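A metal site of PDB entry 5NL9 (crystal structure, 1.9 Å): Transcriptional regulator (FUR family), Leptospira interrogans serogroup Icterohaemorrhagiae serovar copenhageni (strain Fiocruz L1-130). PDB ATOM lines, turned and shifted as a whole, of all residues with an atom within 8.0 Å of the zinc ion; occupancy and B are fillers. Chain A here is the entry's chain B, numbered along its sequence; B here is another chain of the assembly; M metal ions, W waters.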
ATOM      1  N   ILE A  94     -27.626  -5.600 -26.862  1.00  0.00           N
ATOM      2  CA  ILE A  94     -26.770  -5.554 -25.665  1.00  0.00           C
ATOM      3  C   ILE A  94     -27.756  -5.298 -24.542  1.00  0.00           C
ATOM      4  O   ILE A  94     -28.411  -4.242 -24.516  1.00  0.00           O
ATOM      5  CB  ILE A  94     -25.680  -4.418 -25.803  1.00  0.00           C
ATOM      6  CG1 ILE A  94     -24.578  -4.834 -26.822  1.00  0.00           C
ATOM      7  CG2 ILE A  94     -25.044  -4.038 -24.450  1.00  0.00           C
ATOM      8  CD1 ILE A  94     -23.803  -3.610 -27.500  1.00  0.00           C
ATOM      9  N   HIS A  95     -27.900  -6.267 -23.647  1.00  0.00           N
ATOM     10  CA  HIS A  95     -28.917  -6.164 -22.600  1.00  0.00           C
ATOM     11  C   HIS A  95     -28.414  -5.612 -21.250  1.00  0.00           C
ATOM     12  O   HIS A  95     -29.117  -5.784 -20.266  1.00  0.00           O
ATOM     13  CB  HIS A  95     -29.627  -7.545 -22.388  1.00  0.00           C
ATOM     14  CG  HIS A  95     -30.038  -8.233 -23.661  1.00  0.00           C
ATOM     15  ND1 HIS A  95     -31.219  -7.906 -24.314  1.00  0.00           N
ATOM     16  CD2 HIS A  95     -29.409  -9.212 -24.364  1.00  0.00           C
ATOM     17  CE1 HIS A  95     -31.275  -8.690 -25.379  1.00  0.00           C
ATOM     18  NE2 HIS A  95     -30.207  -9.499 -25.456  1.00  0.00           N
ATOM     19  N   HIS A  96     -27.229  -4.916 -21.212  1.00  0.00           N
ATOM     20  CA  HIS A  96     -26.582  -4.341 -20.006  1.00  0.00           C
ATOM     21  C   HIS A  96     -25.968  -2.957 -20.345  1.00  0.00           C
ATOM     22  O   HIS A  96     -25.995  -2.545 -21.501  1.00  0.00           O
ATOM     23  CB  HIS A  96     -25.453  -5.295 -19.495  1.00  0.00           C
ATOM     24  CG  HIS A  96     -24.389  -5.574 -20.510  1.00  0.00           C
ATOM     25  ND1 HIS A  96     -24.541  -6.570 -21.466  1.00  0.00           N
ATOM     26  CD2 HIS A  96     -23.216  -4.933 -20.740  1.00  0.00           C
ATOM     27  CE1 HIS A  96     -23.433  -6.543 -22.190  1.00  0.00           C
ATOM     28  NE2 HIS A  96     -22.609  -5.562 -21.799  1.00  0.00           N
ATOM     29  N   HIS A  97     -25.446  -2.252 -19.338  1.00  0.00           N
ATOM     30  CA  HIS A  97     -24.831  -0.923 -19.526  1.00  0.00           C
ATOM     31  C   HIS A  97     -23.334  -1.038 -19.288  1.00  0.00           C
ATOM     32  O   HIS A  97     -22.833  -2.148 -19.064  1.00  0.00           O
ATOM     33  CB  HIS A  97     -25.490   0.136 -18.628  1.00  0.00           C
ATOM     34  CG  HIS A  97     -26.955   0.194 -18.856  1.00  0.00           C
ATOM     35  ND1 HIS A  97     -27.467   0.558 -20.083  1.00  0.00           N
ATOM     36  CD2 HIS A  97     -27.971  -0.193 -18.063  1.00  0.00           C
ATOM     37  CE1 HIS A  97     -28.771   0.431 -19.991  1.00  0.00           C
ATOM     38  NE2 HIS A  97     -29.139  -0.020 -18.779  1.00  0.00           N
ATOM     39  N   HIS A  98     -22.631   0.098 -19.359  1.00  0.00           N
ATOM     40  CA  HIS A  98     -21.167   0.091 -19.248  1.00  0.00           C
ATOM     41  C   HIS A  98     -20.594   1.205 -18.426  1.00  0.00           C
ATOM     42  O   HIS A  98     -21.048   2.352 -18.507  1.00  0.00           O
ATOM     43  CB  HIS A  98     -20.548   0.184 -20.647  1.00  0.00           C
ATOM     44  CG  HIS A  98     -20.848  -1.006 -21.479  1.00  0.00           C
ATOM     45  ND1 HIS A  98     -21.937  -1.038 -22.330  1.00  0.00           N
ATOM     46  CD2 HIS A  98     -20.238  -2.219 -21.529  1.00  0.00           C
ATOM     47  CE1 HIS A  98     -21.939  -2.257 -22.871  1.00  0.00           C
ATOM     48  NE2 HIS A  98     -20.920  -2.985 -22.426  1.00  0.00           N
ATOM     49  N   ALA A  99     -19.560   0.886 -17.638  1.00  0.00           N
ATOM     50  CA  ALA A  99     -18.752   1.847 -16.935  1.00  0.00           C
ATOM     51  C   ALA A  99     -17.402   1.820 -17.638  1.00  0.00           C
ATOM     52  O   ALA A  99     -16.915   0.761 -18.012  1.00  0.00           O
ATOM     53  CB  ALA A  99     -18.576   1.460 -15.481  1.00  0.00           C
ATOM     54  N   ILE A 107     -13.427  -1.059 -20.196  1.00  0.00           N
ATOM     55  CA  ILE A 107     -14.885  -1.087 -20.120  1.00  0.00           C
ATOM     56  C   ILE A 107     -15.381  -2.239 -19.226  1.00  0.00           C
ATOM     57  O   ILE A 107     -14.932  -3.376 -19.377  1.00  0.00           O
ATOM     58  CB  ILE A 107     -15.434  -1.223 -21.568  1.00  0.00           C
ATOM     59  CG1 ILE A 107     -15.004  -0.044 -22.435  1.00  0.00           C
ATOM     60  CG2 ILE A 107     -16.932  -1.410 -21.603  1.00  0.00           C
ATOM     61  CD1 ILE A 107     -14.743  -0.460 -23.902  1.00  0.00           C
ATOM     62  N   TYR A 108     -16.333  -1.922 -18.335  1.00  0.00           N
ATOM     63  CA  TYR A 108     -16.952  -2.859 -17.387  1.00  0.00           C
ATOM     64  C   TYR A 108     -18.460  -2.953 -17.609  1.00  0.00           C
ATOM     65  O   TYR A 108     -19.122  -1.915 -17.701  1.00  0.00           O
ATOM     66  CB  TYR A 108     -16.677  -2.420 -15.938  1.00  0.00           C
ATOM     67  CG  TYR A 108     -15.204  -2.294 -15.648  1.00  0.00           C
ATOM     68  CD1 TYR A 108     -14.501  -1.154 -16.022  1.00  0.00           C
ATOM     69  CD2 TYR A 108     -14.481  -3.343 -15.081  1.00  0.00           C
ATOM     70  CE1 TYR A 108     -13.125  -1.063 -15.846  1.00  0.00           C
ATOM     71  CE2 TYR A 108     -13.103  -3.281 -14.915  1.00  0.00           C
ATOM     72  CZ  TYR A 108     -12.425  -2.122 -15.263  1.00  0.00           C
ATOM     73  OH  TYR A 108     -11.086  -2.006 -15.031  1.00  0.00           O
ATOM     74  N   ASP A 109     -19.008  -4.169 -17.611  1.00  0.00           N
ATOM     75  CA  ASP A 109     -20.445  -4.399 -17.745  1.00  0.00           C
ATOM     76  C   ASP A 109     -21.113  -4.094 -16.415  1.00  0.00           C
ATOM     77  O   ASP A 109     -20.590  -4.456 -15.368  1.00  0.00           O
ATOM     78  CB  ASP A 109     -20.699  -5.867 -18.126  1.00  0.00           C
ATOM     79  CG  ASP A 109     -20.402  -6.174 -19.576  1.00  0.00           C
ATOM     80  OD1 ASP A 109     -20.145  -5.203 -20.349  1.00  0.00           O
ATOM     81  OD2 ASP A 109     -20.537  -7.358 -19.972  1.00  0.00           O
ATOM     82  N   ILE A 110     -22.225  -3.349 -16.445  1.00  0.00           N
ATOM     83  CA  ILE A 110     -22.988  -2.956 -15.256  1.00  0.00           C
ATOM     84  C   ILE A 110     -24.473  -2.990 -15.593  1.00  0.00           C
ATOM     85  O   ILE A 110     -24.813  -2.830 -16.758  1.00  0.00           O
ATOM     86  CB  ILE A 110     -22.494  -1.632 -14.601  1.00  0.00           C
ATOM     87  CG1 ILE A 110     -22.536  -0.419 -15.555  1.00  0.00           C
ATOM     88  CG2 ILE A 110     -21.129  -1.783 -13.930  1.00  0.00           C
ATOM     89  CD1 ILE A 110     -22.337   0.974 -14.827  1.00  0.00           C
ATOM     90  N   LYS B  83     -22.222   4.555 -31.578  1.00  0.00           N
ATOM     91  CA  LYS B  83     -21.838   3.136 -31.633  1.00  0.00           C
ATOM     92  C   LYS B  83     -21.692   2.604 -33.095  1.00  0.00           C
ATOM     93  O   LYS B  83     -22.557   1.879 -33.603  1.00  0.00           O
ATOM     94  CB  LYS B  83     -22.764   2.266 -30.762  1.00  0.00           C
ATOM     95  CG  LYS B  83     -22.665   2.524 -29.257  1.00  0.00           C
ATOM     96  CD  LYS B  83     -21.599   1.660 -28.543  1.00  0.00           C
ATOM     97  CE  LYS B  83     -21.599   1.816 -27.043  1.00  0.00           C
ATOM     98  NZ  LYS B  83     -22.662   1.014 -26.385  1.00  0.00           N
HETATM   99 ZN    ZN M   1     -20.629  -5.089 -22.448  1.00  0.00          ZN
HETATM  100  O   HOH W   1     -20.313  -7.187 -22.639  1.00  0.00           O
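Three residues have an atom within 4 Å of the zinc ion: His 96, His 98 and Asp 109. The nearest printed residue that does not touch the zinc ion is Ile 94 (5.0 Å).
The zinc ion is bound by NE2 of His 98 (2.1 Å). Water W1 binds the zinc ion. NE2 of His 96 is bound to the zinc ion, 2.1 Å away. OD1 of Asp 109 is bound to the zinc ion (2.2 Å). The zinc ion has four donor atoms within binding distance.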
